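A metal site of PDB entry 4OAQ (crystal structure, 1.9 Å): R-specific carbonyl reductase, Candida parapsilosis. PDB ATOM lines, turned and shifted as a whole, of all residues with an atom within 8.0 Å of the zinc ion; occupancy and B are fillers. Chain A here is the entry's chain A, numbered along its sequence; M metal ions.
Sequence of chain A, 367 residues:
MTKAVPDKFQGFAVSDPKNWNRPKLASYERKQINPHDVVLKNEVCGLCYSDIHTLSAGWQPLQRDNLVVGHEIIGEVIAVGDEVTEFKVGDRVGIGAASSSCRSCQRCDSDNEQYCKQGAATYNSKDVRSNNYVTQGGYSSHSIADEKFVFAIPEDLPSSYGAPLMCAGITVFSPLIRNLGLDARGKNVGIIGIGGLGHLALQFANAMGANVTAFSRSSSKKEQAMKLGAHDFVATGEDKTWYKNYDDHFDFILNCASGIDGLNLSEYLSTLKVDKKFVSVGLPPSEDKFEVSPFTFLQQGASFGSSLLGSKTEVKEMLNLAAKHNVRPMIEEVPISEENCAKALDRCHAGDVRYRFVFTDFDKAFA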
ATOM      1  N   SER A 100      18.339 -16.976  -2.154  1.00  0.00           N
ATOM      2  CA  SER A 100      18.273 -17.508  -0.798  1.00  0.00           C
ATOM      3  C   SER A 100      18.749 -18.959  -0.690  1.00  0.00           C
ATOM      4  O   SER A 100      18.829 -19.680  -1.702  1.00  0.00           O
ATOM      5  CB  SER A 100      16.850 -17.367  -0.234  1.00  0.00           C
ATOM      6  OG  SER A 100      15.905 -18.027  -1.070  1.00  0.00           O
ATOM      7  N   SER A 101      19.070 -19.363   0.544  1.00  0.00           N
ATOM      8  CA  SER A 101      19.554 -20.701   0.866  1.00  0.00           C
ATOM      9  C   SER A 101      18.982 -21.136   2.212  1.00  0.00           C
ATOM     10  O   SER A 101      18.259 -20.379   2.843  1.00  0.00           O
ATOM     11  CB  SER A 101      21.077 -20.738   0.853  1.00  0.00           C
ATOM     12  OG  SER A 101      21.636 -19.930   1.876  1.00  0.00           O
ATOM     13  N   CYS A 102      19.286 -22.350   2.660  1.00  0.00           N
ATOM     14  CA  CYS A 102      18.618 -22.850   3.862  1.00  0.00           C
ATOM     15  C   CYS A 102      19.152 -22.303   5.198  1.00  0.00           C
ATOM     16  O   CYS A 102      18.452 -22.363   6.220  1.00  0.00           O
ATOM     17  CB  CYS A 102      18.640 -24.386   3.874  1.00  0.00           C
ATOM     18  SG  CYS A 102      20.203 -25.164   4.388  1.00  0.00           S
ATOM     19  N   ARG A 103      20.372 -21.771   5.202  1.00  0.00           N
ATOM     20  CA  ARG A 103      21.016 -21.311   6.445  1.00  0.00           C
ATOM     21  C   ARG A 103      21.228 -22.415   7.477  1.00  0.00           C
ATOM     22  O   ARG A 103      21.428 -22.127   8.667  1.00  0.00           O
ATOM     23  CB  ARG A 103      20.232 -20.147   7.065  1.00  0.00           C
ATOM     24  CG  ARG A 103      20.375 -18.844   6.292  1.00  0.00           C
ATOM     25  CD  ARG A 103      19.624 -17.706   6.961  1.00  0.00           C
ATOM     26  NE  ARG A 103      19.907 -16.471   6.242  1.00  0.00           N
ATOM     27  CZ  ARG A 103      20.919 -15.669   6.563  1.00  0.00           C
ATOM     28  NH1 ARG A 103      21.687 -15.975   7.593  1.00  0.00           N
ATOM     29  NH2 ARG A 103      21.143 -14.565   5.860  1.00  0.00           N
ATOM     30  N   SER A 104      21.183 -23.676   7.051  1.00  0.00           N
ATOM     31  CA  SER A 104      21.278 -24.780   8.005  1.00  0.00           C
ATOM     32  C   SER A 104      21.919 -26.016   7.401  1.00  0.00           C
ATOM     33  O   SER A 104      21.564 -27.137   7.746  1.00  0.00           O
ATOM     34  CB  SER A 104      19.906 -25.133   8.569  1.00  0.00           C
ATOM     35  OG  SER A 104      19.251 -26.080   7.749  1.00  0.00           O
ATOM     36  N   CYS A 105      22.884 -25.816   6.515  1.00  0.00           N
ATOM     37  CA  CYS A 105      23.649 -26.922   5.984  1.00  0.00           C
ATOM     38  C   CYS A 105      25.118 -26.516   5.965  1.00  0.00           C
ATOM     39  O   CYS A 105      25.444 -25.363   6.226  1.00  0.00           O
ATOM     40  CB  CYS A 105      23.176 -27.285   4.579  1.00  0.00           C
ATOM     41  SG  CYS A 105      23.669 -26.113   3.293  1.00  0.00           S
ATOM     42  N   GLN A 106      25.989 -27.459   5.650  1.00  0.00           N
ATOM     43  CA  GLN A 106      27.412 -27.170   5.686  1.00  0.00           C
ATOM     44  C   GLN A 106      27.835 -26.217   4.579  1.00  0.00           C
ATOM     45  O   GLN A 106      28.642 -25.328   4.823  1.00  0.00           O
ATOM     46  CB  GLN A 106      28.256 -28.444   5.640  1.00  0.00           C
ATOM     47  CG  GLN A 106      29.739 -28.205   5.873  1.00  0.00           C
ATOM     48  CD  GLN A 106      30.058 -27.599   7.236  1.00  0.00           C
ATOM     49  OE1 GLN A 106      29.544 -28.046   8.267  1.00  0.00           O
ATOM     50  NE2 GLN A 106      30.918 -26.577   7.248  1.00  0.00           N
ATOM     51  N   ARG A 107      27.311 -26.410   3.372  1.00  0.00           N
ATOM     52  CA  ARG A 107      27.541 -25.493   2.253  1.00  0.00           C
ATOM     53  C   ARG A 107      27.217 -24.047   2.580  1.00  0.00           C
ATOM     54  O   ARG A 107      27.957 -23.132   2.223  1.00  0.00           O
ATOM     55  CB  ARG A 107      26.745 -25.940   1.014  1.00  0.00           C
ATOM     56  CG  ARG A 107      27.211 -27.278   0.506  1.00  0.00           C
ATOM     57  CD  ARG A 107      26.363 -27.833  -0.601  1.00  0.00           C
ATOM     58  NE  ARG A 107      26.873 -29.140  -1.005  1.00  0.00           N
ATOM     59  CZ  ARG A 107      26.644 -29.728  -2.175  1.00  0.00           C
ATOM     60  NH1 ARG A 107      25.903 -29.121  -3.112  1.00  0.00           N
ATOM     61  NH2 ARG A 107      27.187 -30.901  -2.434  1.00  0.00           N
ATOM     62  N   CYS A 108      26.095 -23.838   3.258  1.00  0.00           N
ATOM     63  CA  CYS A 108      25.702 -22.505   3.641  1.00  0.00           C
ATOM     64  C   CYS A 108      26.697 -21.865   4.602  1.00  0.00           C
ATOM     65  O   CYS A 108      26.842 -20.648   4.606  1.00  0.00           O
ATOM     66  CB  CYS A 108      24.302 -22.529   4.281  1.00  0.00           C
ATOM     67  SG  CYS A 108      22.961 -22.536   3.051  1.00  0.00           S
ATOM     68  N   ASP A 109      27.404 -22.669   5.388  1.00  0.00           N
ATOM     69  CA  ASP A 109      28.359 -22.107   6.349  1.00  0.00           C
ATOM     70  C   ASP A 109      29.822 -22.218   5.906  1.00  0.00           C
ATOM     71  O   ASP A 109      30.728 -21.985   6.707  1.00  0.00           O
ATOM     72  CB  ASP A 109      28.182 -22.756   7.732  1.00  0.00           C
ATOM     73  N   ASN A 112      29.744 -21.985   0.225  1.00  0.00           N
ATOM     74  CA  ASN A 112      29.169 -22.690  -0.913  1.00  0.00           C
ATOM     75  C   ASN A 112      27.660 -22.535  -0.922  1.00  0.00           C
ATOM     76  O   ASN A 112      26.928 -23.409  -1.397  1.00  0.00           O
ATOM     77  CB  ASN A 112      29.588 -24.166  -0.913  1.00  0.00           C
ATOM     78  CG  ASN A 112      30.876 -24.396  -1.675  1.00  0.00           C
ATOM     79  OD1 ASN A 112      31.114 -23.761  -2.696  1.00  0.00           O
ATOM     80  ND2 ASN A 112      31.707 -25.304  -1.183  1.00  0.00           N
ATOM     81  N   GLU A 113      27.197 -21.389  -0.435  1.00  0.00           N
ATOM     82  CA  GLU A 113      25.767 -21.174  -0.262  1.00  0.00           C
ATOM     83  C   GLU A 113      25.031 -21.185  -1.610  1.00  0.00           C
ATOM     84  O   GLU A 113      23.820 -21.399  -1.651  1.00  0.00           O
ATOM     85  CB  GLU A 113      25.506 -19.875   0.518  1.00  0.00           C
ATOM     86  CG  GLU A 113      25.953 -18.587  -0.201  1.00  0.00           C
ATOM     87  CD  GLU A 113      27.422 -18.222   0.051  1.00  0.00           C
ATOM     88  OE1 GLU A 113      28.148 -19.024   0.686  1.00  0.00           O
ATOM     89  OE2 GLU A 113      27.854 -17.115  -0.352  1.00  0.00           O
ATOM     90  N   GLN A 114      25.756 -20.975  -2.703  1.00  0.00           N
ATOM     91  CA  GLN A 114      25.122 -20.972  -4.029  1.00  0.00           C
ATOM     92  C   GLN A 114      24.814 -22.417  -4.401  1.00  0.00           C
ATOM     93  O   GLN A 114      23.968 -22.690  -5.231  1.00  0.00           O
ATOM     94  CB  GLN A 114      26.030 -20.292  -5.087  1.00  0.00           C
ATOM     95  CG  GLN A 114      27.316 -21.083  -5.497  1.00  0.00           C
ATOM     96  CD  GLN A 114      28.505 -20.864  -4.551  1.00  0.00           C
ATOM     97  OE1 GLN A 114      28.336 -20.450  -3.399  1.00  0.00           O
ATOM     98  NE2 GLN A 114      29.719 -21.147  -5.044  1.00  0.00           N
ATOM     99  N   TYR A 115      25.494 -23.355  -3.747  1.00  0.00           N
ATOM    100  CA  TYR A 115      25.204 -24.786  -3.922  1.00  0.00           C
ATOM    101  C   TYR A 115      24.246 -25.378  -2.899  1.00  0.00           C
ATOM    102  O   TYR A 115      24.131 -26.602  -2.801  1.00  0.00           O
ATOM    103  CB  TYR A 115      26.493 -25.596  -3.925  1.00  0.00           C
ATOM    104  CG  TYR A 115      27.343 -25.353  -5.162  1.00  0.00           C
ATOM    105  CD1 TYR A 115      26.973 -25.880  -6.393  1.00  0.00           C
ATOM    106  CD2 TYR A 115      28.521 -24.623  -5.092  1.00  0.00           C
ATOM    107  CE1 TYR A 115      27.757 -25.667  -7.529  1.00  0.00           C
ATOM    108  CE2 TYR A 115      29.306 -24.402  -6.221  1.00  0.00           C
ATOM    109  CZ  TYR A 115      28.911 -24.920  -7.428  1.00  0.00           C
ATOM    110  OH  TYR A 115      29.669 -24.704  -8.547  1.00  0.00           O
ATOM    111  N   CYS A 116      23.578 -24.541  -2.115  1.00  0.00           N
ATOM    112  CA  CYS A 116      22.615 -25.102  -1.151  1.00  0.00           C
ATOM    113  C   CYS A 116      21.584 -25.960  -1.870  1.00  0.00           C
ATOM    114  O   CYS A 116      21.049 -25.562  -2.897  1.00  0.00           O
ATOM    115  CB  CYS A 116      21.900 -24.007  -0.375  1.00  0.00           C
ATOM    116  SG  CYS A 116      20.826 -24.677   0.880  1.00  0.00           S
ATOM    117  N   LYS A 117      21.322 -27.148  -1.334  1.00  0.00           N
ATOM    118  CA  LYS A 117      20.382 -28.068  -1.951  1.00  0.00           C
ATOM    119  C   LYS A 117      18.983 -27.466  -1.988  1.00  0.00           C
ATOM    120  O   LYS A 117      18.167 -27.798  -2.852  1.00  0.00           O
ATOM    121  CB  LYS A 117      20.372 -29.366  -1.167  1.00  0.00           C
ATOM    122  CG  LYS A 117      19.463 -30.427  -1.735  1.00  0.00           C
ATOM    123  CD  LYS A 117      19.544 -31.657  -0.879  1.00  0.00           C
ATOM    124  N   GLN A 118      18.695 -26.579  -1.060  1.00  0.00           N
ATOM    125  CA  GLN A 118      17.388 -25.932  -1.003  1.00  0.00           C
ATOM    126  C   GLN A 118      17.495 -24.471  -1.454  1.00  0.00           C
ATOM    127  O   GLN A 118      16.695 -23.621  -1.075  1.00  0.00           O
ATOM    128  CB  GLN A 118      16.804 -26.028   0.405  1.00  0.00           C
ATOM    129  CG  GLN A 118      16.751 -27.458   0.957  1.00  0.00           C
ATOM    130  CD  GLN A 118      16.130 -27.529   2.334  1.00  0.00           C
ATOM    131  OE1 GLN A 118      15.556 -26.550   2.825  1.00  0.00           O
ATOM    132  NE2 GLN A 118      16.246 -28.680   2.971  1.00  0.00           N
ATOM    133  N   GLY A 119      18.508 -24.189  -2.262  1.00  0.00           N
ATOM    134  CA  GLY A 119      18.707 -22.839  -2.777  1.00  0.00           C
ATOM    135  C   GLY A 119      17.505 -22.393  -3.602  1.00  0.00           C
ATOM    136  O   GLY A 119      16.796 -23.224  -4.169  1.00  0.00           O
ATOM    137  N   ARG A 129      11.065 -21.407   1.708  1.00  0.00           N
ATOM    138  CA  ARG A 129      11.085 -20.646   2.946  1.00  0.00           C
ATOM    139  C   ARG A 129      10.077 -19.521   2.918  1.00  0.00           C
ATOM    140  O   ARG A 129       9.846 -18.866   3.925  1.00  0.00           O
ATOM    141  CB  ARG A 129      12.490 -20.076   3.205  1.00  0.00           C
ATOM    142  CG  ARG A 129      13.528 -21.152   3.509  1.00  0.00           C
ATOM    143  CD  ARG A 129      14.966 -20.615   3.349  1.00  0.00           C
ATOM    144  NE  ARG A 129      15.269 -20.304   1.952  1.00  0.00           N
ATOM    145  CZ  ARG A 129      15.623 -21.210   1.044  1.00  0.00           C
ATOM    146  NH1 ARG A 129      15.716 -22.501   1.382  1.00  0.00           N
ATOM    147  NH2 ARG A 129      15.880 -20.828  -0.185  1.00  0.00           N
ATOM    148  N   LYS A 148      22.543 -13.022   2.591  1.00  0.00           N
ATOM    149  CA  LYS A 148      23.673 -13.811   2.111  1.00  0.00           C
ATOM    150  C   LYS A 148      23.851 -13.706   0.604  1.00  0.00           C
ATOM    151  O   LYS A 148      24.889 -14.077   0.065  1.00  0.00           O
ATOM    152  CB  LYS A 148      23.508 -15.286   2.516  1.00  0.00           C
ATOM    153  CG  LYS A 148      23.900 -15.625   3.972  1.00  0.00           C
ATOM    154  CD  LYS A 148      23.579 -17.078   4.315  1.00  0.00           C
ATOM    155  CE  LYS A 148      24.842 -17.918   4.578  1.00  0.00           C
ATOM    156  NZ  LYS A 148      25.591 -17.484   5.798  1.00  0.00           N
ATOM    157  N   PHE A 149      22.829 -13.190  -0.085  1.00  0.00           N
ATOM    158  CA  PHE A 149      22.837 -13.106  -1.536  1.00  0.00           C
ATOM    159  C   PHE A 149      22.775 -11.667  -2.045  1.00  0.00           C
ATOM    160  O   PHE A 149      22.514 -11.422  -3.218  1.00  0.00           O
ATOM    161  CB  PHE A 149      21.732 -13.988  -2.115  1.00  0.00           C
ATOM    162  CG  PHE A 149      21.970 -15.465  -1.904  1.00  0.00           C
ATOM    163  CD1 PHE A 149      22.689 -16.202  -2.828  1.00  0.00           C
ATOM    164  CD2 PHE A 149      21.532 -16.093  -0.749  1.00  0.00           C
ATOM    165  CE1 PHE A 149      22.943 -17.563  -2.609  1.00  0.00           C
ATOM    166  CE2 PHE A 149      21.777 -17.434  -0.520  1.00  0.00           C
ATOM    167  CZ  PHE A 149      22.476 -18.181  -1.443  1.00  0.00           C
HETATM  168 ZN    ZN M   1      21.960 -24.612   2.941  1.00  0.00          ZN
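The backbone NH of Gln 118 lies close to the side-chain sulfur of Cys 116, 3.5 Å away.
The side-chain sulfur of Cys 108 lies close to the backbone NH of Arg 103 (3.5 Å).
The side-chain sulfur of Cys 102 lies close to the backbone NH of Ser 104 (3.2 Å).
SG of Cys 105 lies close to N of Arg 107 (3.7 Å).
The side-chain sulfur (SG) of Cys 108 sits close to the side-chain hydroxyl (OG) of Ser 101 (3.2 Å).
SG of Cys 105 is bound to the zinc ion (2.3 Å).
The zinc ion is bound by SG of Cys 108.
SG of Cys 102 is bound to the zinc ion (2.3 Å).
SG of Cys 116 binds the zinc ion, at 2.4 Å.
Merely in contact with the zinc ion: Arg 103 (3.96 Å).
Of the 21 residues printed, 5 come within 4 Å of the zinc ion.
The nearest printed residue that does not touch the zinc ion is Ser 104 (4.3 Å).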
